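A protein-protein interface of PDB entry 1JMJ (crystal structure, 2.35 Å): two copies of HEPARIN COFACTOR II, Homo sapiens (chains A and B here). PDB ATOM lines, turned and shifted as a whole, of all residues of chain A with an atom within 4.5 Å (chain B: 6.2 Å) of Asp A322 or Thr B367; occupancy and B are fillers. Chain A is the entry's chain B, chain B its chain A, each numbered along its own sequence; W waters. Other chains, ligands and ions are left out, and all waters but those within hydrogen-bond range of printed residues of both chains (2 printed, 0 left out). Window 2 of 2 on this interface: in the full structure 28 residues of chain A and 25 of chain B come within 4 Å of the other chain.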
ATOM      1  N   ASN A 317      -7.123  28.889  30.724  1.00  0.00           N
ATOM      2  CA  ASN A 317      -8.297  29.016  29.889  1.00  0.00           C
ATOM      3  C   ASN A 317      -7.837  29.577  28.560  1.00  0.00           C
ATOM      4  O   ASN A 317      -7.023  30.500  28.521  1.00  0.00           O
ATOM      5  CB  ASN A 317      -9.293  29.977  30.547  1.00  0.00           C
ATOM      6  CG  ASN A 317     -10.539  30.183  29.718  1.00  0.00           C
ATOM      7  OD1 ASN A 317     -10.997  31.317  29.534  1.00  0.00           O
ATOM      8  ND2 ASN A 317     -11.107  29.088  29.217  1.00  0.00           N
ATOM      9  N   ASP A 318      -8.340  29.003  27.475  1.00  0.00           N
ATOM     10  CA  ASP A 318      -7.992  29.466  26.140  1.00  0.00           C
ATOM     11  C   ASP A 318      -9.276  29.970  25.488  1.00  0.00           C
ATOM     12  O   ASP A 318     -10.147  29.182  25.119  1.00  0.00           O
ATOM     13  CB  ASP A 318      -7.399  28.328  25.309  1.00  0.00           C
ATOM     14  CG  ASP A 318      -6.739  28.824  24.035  1.00  0.00           C
ATOM     15  OD1 ASP A 318      -7.288  29.748  23.394  1.00  0.00           O
ATOM     16  OD2 ASP A 318      -5.674  28.285  23.666  1.00  0.00           O
ATOM     17  N   GLN A 319      -9.383  31.285  25.349  1.00  0.00           N
ATOM     18  CA  GLN A 319     -10.569  31.897  24.765  1.00  0.00           C
ATOM     19  C   GLN A 319     -10.679  31.691  23.250  1.00  0.00           C
ATOM     20  O   GLN A 319     -11.770  31.435  22.745  1.00  0.00           O
ATOM     21  CB  GLN A 319     -10.589  33.383  25.132  1.00  0.00           C
ATOM     22  CG  GLN A 319     -11.851  34.141  24.757  1.00  0.00           C
ATOM     23  CD  GLN A 319     -11.928  34.443  23.278  1.00  0.00           C
ATOM     24  OE1 GLN A 319     -10.918  34.756  22.643  1.00  0.00           O
ATOM     25  NE2 GLN A 319     -13.131  34.369  22.720  1.00  0.00           N
ATOM     26  N   GLU A 320      -9.561  31.785  22.528  1.00  0.00           N
ATOM     27  CA  GLU A 320      -9.562  31.585  21.073  1.00  0.00           C
ATOM     28  C   GLU A 320     -10.022  30.182  20.671  1.00  0.00           C
ATOM     29  O   GLU A 320     -10.870  30.022  19.796  1.00  0.00           O
ATOM     30  CB  GLU A 320      -8.166  31.783  20.497  1.00  0.00           C
ATOM     31  CG  GLU A 320      -7.536  33.116  20.775  1.00  0.00           C
ATOM     32  CD  GLU A 320      -6.033  33.070  20.577  1.00  0.00           C
ATOM     33  OE1 GLU A 320      -5.595  32.722  19.453  1.00  0.00           O
ATOM     34  OE2 GLU A 320      -5.294  33.373  21.544  1.00  0.00           O
ATOM     35  N   LEU A 321      -9.437  29.162  21.290  1.00  0.00           N
ATOM     36  CA  LEU A 321      -9.800  27.785  20.970  1.00  0.00           C
ATOM     37  C   LEU A 321     -10.949  27.299  21.850  1.00  0.00           C
ATOM     38  O   LEU A 321     -11.515  26.230  21.615  1.00  0.00           O
ATOM     39  CB  LEU A 321      -8.586  26.862  21.149  1.00  0.00           C
ATOM     40  CG  LEU A 321      -7.336  27.254  20.363  1.00  0.00           C
ATOM     41  CD1 LEU A 321      -6.259  26.203  20.528  1.00  0.00           C
ATOM     42  CD2 LEU A 321      -7.694  27.411  18.905  1.00  0.00           C
ATOM     43  N   ASP A 322     -11.297  28.103  22.851  1.00  0.00           N
ATOM     44  CA  ASP A 322     -12.346  27.767  23.805  1.00  0.00           C
ATOM     45  C   ASP A 322     -12.102  26.373  24.377  1.00  0.00           C
ATOM     46  O   ASP A 322     -12.864  25.424  24.152  1.00  0.00           O
ATOM     47  CB  ASP A 322     -13.738  27.858  23.166  1.00  0.00           C
ATOM     48  CG  ASP A 322     -14.858  27.874  24.210  1.00  0.00           C
ATOM     49  OD1 ASP A 322     -14.586  28.232  25.381  1.00  0.00           O
ATOM     50  OD2 ASP A 322     -16.014  27.548  23.865  1.00  0.00           O
ATOM     51  N   CYS A 323     -11.009  26.274  25.116  1.00  0.00           N
ATOM     52  CA  CYS A 323     -10.596  25.041  25.761  1.00  0.00           C
ATOM     53  C   CYS A 323     -10.153  25.354  27.171  1.00  0.00           C
ATOM     54  O   CYS A 323      -9.793  26.486  27.482  1.00  0.00           O
ATOM     55  CB  CYS A 323      -9.398  24.419  25.035  1.00  0.00           C
ATOM     56  SG  CYS A 323      -9.765  23.672  23.457  1.00  0.00           S
ATOM     57  N   VAL A 340      -9.375  20.216  27.286  1.00  0.00           N
ATOM     58  CA  VAL A 340     -10.792  19.948  27.039  1.00  0.00           C
ATOM     59  C   VAL A 340     -11.522  21.048  26.255  1.00  0.00           C
ATOM     60  O   VAL A 340     -11.867  22.086  26.815  1.00  0.00           O
ATOM     61  CB  VAL A 340     -11.563  19.743  28.382  1.00  0.00           C
ATOM     62  CG1 VAL A 340     -12.891  19.076  28.117  1.00  0.00           C
ATOM     63  CG2 VAL A 340     -10.735  18.907  29.354  1.00  0.00           C
ATOM     64  N   PRO A 341     -11.741  20.849  24.942  1.00  0.00           N
ATOM     65  CA  PRO A 341     -12.454  21.917  24.235  1.00  0.00           C
ATOM     66  C   PRO A 341     -13.887  21.962  24.763  1.00  0.00           C
ATOM     67  O   PRO A 341     -14.462  20.925  25.082  1.00  0.00           O
ATOM     68  CB  PRO A 341     -12.353  21.502  22.761  1.00  0.00           C
ATOM     69  CG  PRO A 341     -12.122  20.020  22.807  1.00  0.00           C
ATOM     70  CD  PRO A 341     -11.224  19.836  24.002  1.00  0.00           C
ATOM     71  N   HIS A 342     -14.446  23.163  24.882  1.00  0.00           N
ATOM     72  CA  HIS A 342     -15.798  23.321  25.405  1.00  0.00           C
ATOM     73  C   HIS A 342     -16.872  22.719  24.504  1.00  0.00           C
ATOM     74  O   HIS A 342     -17.820  22.094  24.986  1.00  0.00           O
ATOM     75  CB  HIS A 342     -16.098  24.806  25.644  1.00  0.00           C
ATOM     76  CG  HIS A 342     -17.490  25.075  26.126  1.00  0.00           C
ATOM     77  ND1 HIS A 342     -18.034  24.444  27.228  1.00  0.00           N
ATOM     78  CD2 HIS A 342     -18.451  25.910  25.663  1.00  0.00           C
ATOM     79  CE1 HIS A 342     -19.265  24.879  27.420  1.00  0.00           C
ATOM     80  NE2 HIS A 342     -19.543  25.771  26.485  1.00  0.00           N
ATOM     81  N   LYS A 343     -16.713  22.891  23.198  1.00  0.00           N
ATOM     82  CA  LYS A 343     -17.689  22.381  22.242  1.00  0.00           C
ATOM     83  C   LYS A 343     -17.188  21.191  21.436  1.00  0.00           C
ATOM     84  O   LYS A 343     -15.986  21.036  21.214  1.00  0.00           O
ATOM     85  CB  LYS A 343     -18.094  23.493  21.275  1.00  0.00           C
ATOM     86  CG  LYS A 343     -18.500  24.775  21.957  1.00  0.00           C
ATOM     87  CD  LYS A 343     -19.176  25.707  20.977  1.00  0.00           C
ATOM     88  CE  LYS A 343     -19.587  26.987  21.671  1.00  0.00           C
ATOM     89  NZ  LYS A 343     -20.343  27.886  20.757  1.00  0.00           N
ATOM     90  N   PHE B 313     -22.652  31.024  32.962  1.00  0.00           N
ATOM     91  CA  PHE B 313     -22.011  32.265  33.359  1.00  0.00           C
ATOM     92  C   PHE B 313     -20.735  32.432  32.560  1.00  0.00           C
ATOM     93  O   PHE B 313     -20.070  31.448  32.246  1.00  0.00           O
ATOM     94  CB  PHE B 313     -21.608  32.220  34.838  1.00  0.00           C
ATOM     95  CG  PHE B 313     -22.731  31.938  35.789  1.00  0.00           C
ATOM     96  CD1 PHE B 313     -23.481  32.982  36.329  1.00  0.00           C
ATOM     97  CD2 PHE B 313     -22.999  30.632  36.199  1.00  0.00           C
ATOM     98  CE1 PHE B 313     -24.485  32.728  37.278  1.00  0.00           C
ATOM     99  CE2 PHE B 313     -23.993  30.360  37.141  1.00  0.00           C
ATOM    100  CZ  PHE B 313     -24.740  31.409  37.687  1.00  0.00           C
ATOM    101  N   LEU B 314     -20.395  33.675  32.230  1.00  0.00           N
ATOM    102  CA  LEU B 314     -19.136  33.937  31.553  1.00  0.00           C
ATOM    103  C   LEU B 314     -18.150  34.158  32.701  1.00  0.00           C
ATOM    104  O   LEU B 314     -18.507  34.731  33.738  1.00  0.00           O
ATOM    105  CB  LEU B 314     -19.221  35.200  30.694  1.00  0.00           C
ATOM    106  CG  LEU B 314     -20.176  35.110  29.498  1.00  0.00           C
ATOM    107  CD1 LEU B 314     -20.147  36.415  28.715  1.00  0.00           C
ATOM    108  CD2 LEU B 314     -19.773  33.941  28.602  1.00  0.00           C
ATOM    109  N   ALA B 315     -16.923  33.683  32.534  1.00  0.00           N
ATOM    110  CA  ALA B 315     -15.890  33.859  33.557  1.00  0.00           C
ATOM    111  C   ALA B 315     -14.518  33.999  32.901  1.00  0.00           C
ATOM    112  O   ALA B 315     -14.354  33.721  31.717  1.00  0.00           O
ATOM    113  CB  ALA B 315     -15.897  32.667  34.531  1.00  0.00           C
ATOM    114  N   ALA B 316     -13.536  34.440  33.679  1.00  0.00           N
ATOM    115  CA  ALA B 316     -12.179  34.608  33.175  1.00  0.00           C
ATOM    116  C   ALA B 316     -11.174  34.647  34.320  1.00  0.00           C
ATOM    117  O   ALA B 316     -11.522  34.947  35.466  1.00  0.00           O
ATOM    118  CB  ALA B 316     -12.077  35.896  32.360  1.00  0.00           C
ATOM    119  N   GLN B 363     -12.875  41.106  29.874  1.00  0.00           N
ATOM    120  CA  GLN B 363     -14.026  40.956  28.992  1.00  0.00           C
ATOM    121  C   GLN B 363     -13.714  40.141  27.744  1.00  0.00           C
ATOM    122  O   GLN B 363     -14.482  39.259  27.362  1.00  0.00           O
ATOM    123  CB  GLN B 363     -14.562  42.332  28.578  1.00  0.00           C
ATOM    124  CG  GLN B 363     -15.374  43.037  29.648  1.00  0.00           C
ATOM    125  CD  GLN B 363     -16.722  42.370  29.895  1.00  0.00           C
ATOM    126  OE1 GLN B 363     -17.459  42.751  30.811  1.00  0.00           O
ATOM    127  NE2 GLN B 363     -17.057  41.373  29.072  1.00  0.00           N
ATOM    128  N   SER B 365     -11.349  37.920  27.308  1.00  0.00           N
ATOM    129  CA  SER B 365     -10.867  36.560  27.552  1.00  0.00           C
ATOM    130  C   SER B 365     -11.926  35.712  28.237  1.00  0.00           C
ATOM    131  O   SER B 365     -11.674  34.590  28.650  1.00  0.00           O
ATOM    132  CB  SER B 365      -9.606  36.583  28.412  1.00  0.00           C
ATOM    133  OG  SER B 365      -9.899  37.030  29.716  1.00  0.00           O
ATOM    134  N   MET B 366     -13.123  36.261  28.344  1.00  0.00           N
ATOM    135  CA  MET B 366     -14.226  35.570  28.983  1.00  0.00           C
ATOM    136  C   MET B 366     -14.726  34.378  28.176  1.00  0.00           C
ATOM    137  O   MET B 366     -14.689  34.389  26.950  1.00  0.00           O
ATOM    138  CB  MET B 366     -15.370  36.553  29.179  1.00  0.00           C
ATOM    139  CG  MET B 366     -16.117  36.374  30.464  1.00  0.00           C
ATOM    140  SD  MET B 366     -16.074  37.886  31.398  1.00  0.00           S
ATOM    141  CE  MET B 366     -15.261  37.345  32.843  1.00  0.00           C
ATOM    142  N   THR B 367     -15.188  33.343  28.868  1.00  0.00           N
ATOM    143  CA  THR B 367     -15.736  32.174  28.197  1.00  0.00           C
ATOM    144  C   THR B 367     -17.019  31.741  28.902  1.00  0.00           C
ATOM    145  O   THR B 367     -17.195  31.969  30.102  1.00  0.00           O
ATOM    146  CB  THR B 367     -14.733  30.977  28.142  1.00  0.00           C
ATOM    147  OG1 THR B 367     -14.121  30.779  29.427  1.00  0.00           O
ATOM    148  CG2 THR B 367     -13.667  31.234  27.102  1.00  0.00           C
ATOM    149  N   ASN B 368     -17.907  31.128  28.125  1.00  0.00           N
ATOM    150  CA  ASN B 368     -19.202  30.648  28.591  1.00  0.00           C
ATOM    151  C   ASN B 368     -19.071  29.202  29.044  1.00  0.00           C
ATOM    152  O   ASN B 368     -18.539  28.358  28.320  1.00  0.00           O
ATOM    153  CB  ASN B 368     -20.213  30.736  27.450  1.00  0.00           C
ATOM    154  CG  ASN B 368     -21.638  30.649  27.928  1.00  0.00           C
ATOM    155  OD1 ASN B 368     -21.927  30.003  28.936  1.00  0.00           O
ATOM    156  ND2 ASN B 368     -22.539  31.287  27.189  1.00  0.00           N
ATOM    157  N   ARG B 369     -19.597  28.911  30.226  1.00  0.00           N
ATOM    158  CA  ARG B 369     -19.496  27.569  30.791  1.00  0.00           C
ATOM    159  C   ARG B 369     -20.685  27.315  31.726  1.00  0.00           C
ATOM    160  O   ARG B 369     -21.259  28.257  32.271  1.00  0.00           O
ATOM    161  CB  ARG B 369     -18.174  27.486  31.586  1.00  0.00           C
ATOM    162  CG  ARG B 369     -17.287  26.275  31.321  1.00  0.00           C
ATOM    163  CD  ARG B 369     -17.002  26.103  29.845  1.00  0.00           C
ATOM    164  NE  ARG B 369     -15.590  26.167  29.493  1.00  0.00           N
ATOM    165  CZ  ARG B 369     -15.136  26.801  28.411  1.00  0.00           C
ATOM    166  NH1 ARG B 369     -15.989  27.428  27.602  1.00  0.00           N
ATOM    167  NH2 ARG B 369     -13.840  26.785  28.112  1.00  0.00           N
ATOM    168  N   ARG B 371     -21.756  26.591  35.093  1.00  0.00           N
ATOM    169  CA  ARG B 371     -21.078  26.661  36.374  1.00  0.00           C
ATOM    170  C   ARG B 371     -21.949  26.604  37.602  1.00  0.00           C
ATOM    171  O   ARG B 371     -23.037  27.180  37.641  1.00  0.00           O
ATOM    172  CB  ARG B 371     -20.271  27.967  36.474  1.00  0.00           C
ATOM    173  CG  ARG B 371     -19.465  28.363  35.255  1.00  0.00           C
ATOM    174  CD  ARG B 371     -18.917  29.763  35.430  1.00  0.00           C
ATOM    175  NE  ARG B 371     -18.389  30.285  34.176  1.00  0.00           N
ATOM    176  CZ  ARG B 371     -17.207  29.956  33.673  1.00  0.00           C
ATOM    177  NH1 ARG B 371     -16.819  30.466  32.513  1.00  0.00           N
ATOM    178  NH2 ARG B 371     -16.406  29.136  34.339  1.00  0.00           N
HETATM  179  O   HOH W   1      -9.380  33.665  31.007  1.00  0.00           O
HETATM  180  O   HOH W   2     -16.993  30.101  25.758  1.00  0.00           O
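OG1 of Thr B367 is in hydrogen-bond range of OD1 of Asn A317 (3.2 Å). NH1 of Arg B369 is in salt-bridge range of OD1 of Asp A322, 2.7 Å away. The backbone carbonyl oxygen (O) of Asn B368 lies within hydrogen-bond range of a ring nitrogen (NE2) of His A342 (3.3 Å). The side-chain amide oxygen (OD1) of Asn A317 sits close to the backbone carbonyl oxygen (O) of Ser B365, at 3.5 Å.
The backbone carbonyl oxygen of Arg B369 sits at hydrogen-bond distance from the backbone NH of Phe B313, at 3.2 Å. O of Cys A323 lies within hydrogen-bond range of ND2 of Asn A317, 3.4 Å away. O of Thr B367 sits at hydrogen-bond distance from NH1 of Arg B371, 2.9 Å away. N of His A342 is in hydrogen-bond range of O of Asp A322, 2.9 Å away. N of Ala B315 is in hydrogen-bond range of O of Thr B367 (3.0 Å).
Asn A317 touches Arg B369. Gln A319 touches Ser B365 (CG to C, 3.8 Å). Met B366 touches Gln A319 (O to CG, 3.6 Å). CG2 of Thr B367 touches CA of Gln A319, at 3.9 Å. Asp A322 touches Thr B367. CG of His A342 touches NH1 of Arg B369 (3.2 Å).
Of chain B, only Thr B367 and Arg B369 come within 4 Å of Asp A322. Thr B367 touches just these residues of chain A: Asn A317 (3.2 Å), Gln A319 (3.9 Å) and Asp A322 (3.6 Å). Of the printed residues of chain A, Asn B368 touches His A342 (3.3 Å). Of the printed residues of chain B, Asn A317 touches Ser B365, Thr B367 and Arg B369. Of the printed residues of chain A, Met B366 touches Gln A319. Of the printed residues of chain B, His A342 touches Asn B368 and Arg B369. Cys A323 touches none of the printed residues of chain B. Leu B314 touches none of the printed residues of chain A. The nearest residue of chain B that does not touch Asp A322 is Asn B368 (4.9 Å). The nearest printed residue of chain A that does not touch Thr B367 is Asp A318 (4.5 Å). The nearest printed residue of chain B that does not touch Asn A317 is Ala B315 (4.7 Å).
Hydrophobic or aromatic side chains of chain A that line the printed part of chain B: His A342. Of the 11 printed residues of chain B, 5 touch a printed residue of chain A. Printed residues of chain B that touch a printed residue of chain A: Ser B365, Met B366, Thr B367, Asn B368 and Arg B369. Among the printed residues, Asp or Glu carboxylates within 4 Å of a Lys or Arg side-chain nitrogen of the other chain: Asp A322 with Arg B369 (2.7 Å).
No position is printed for both chains.
Water W2 lies within hydrogen-bond range of N of Asn B368, OD1 of Asp A322 and NH1 of Arg B369. Water W1 bridges the side-chain amide oxygen (OD1) of Asn A317 (3.2 Å) and the backbone carbonyl oxygen (O) of Ser B365 (3.4 Å).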
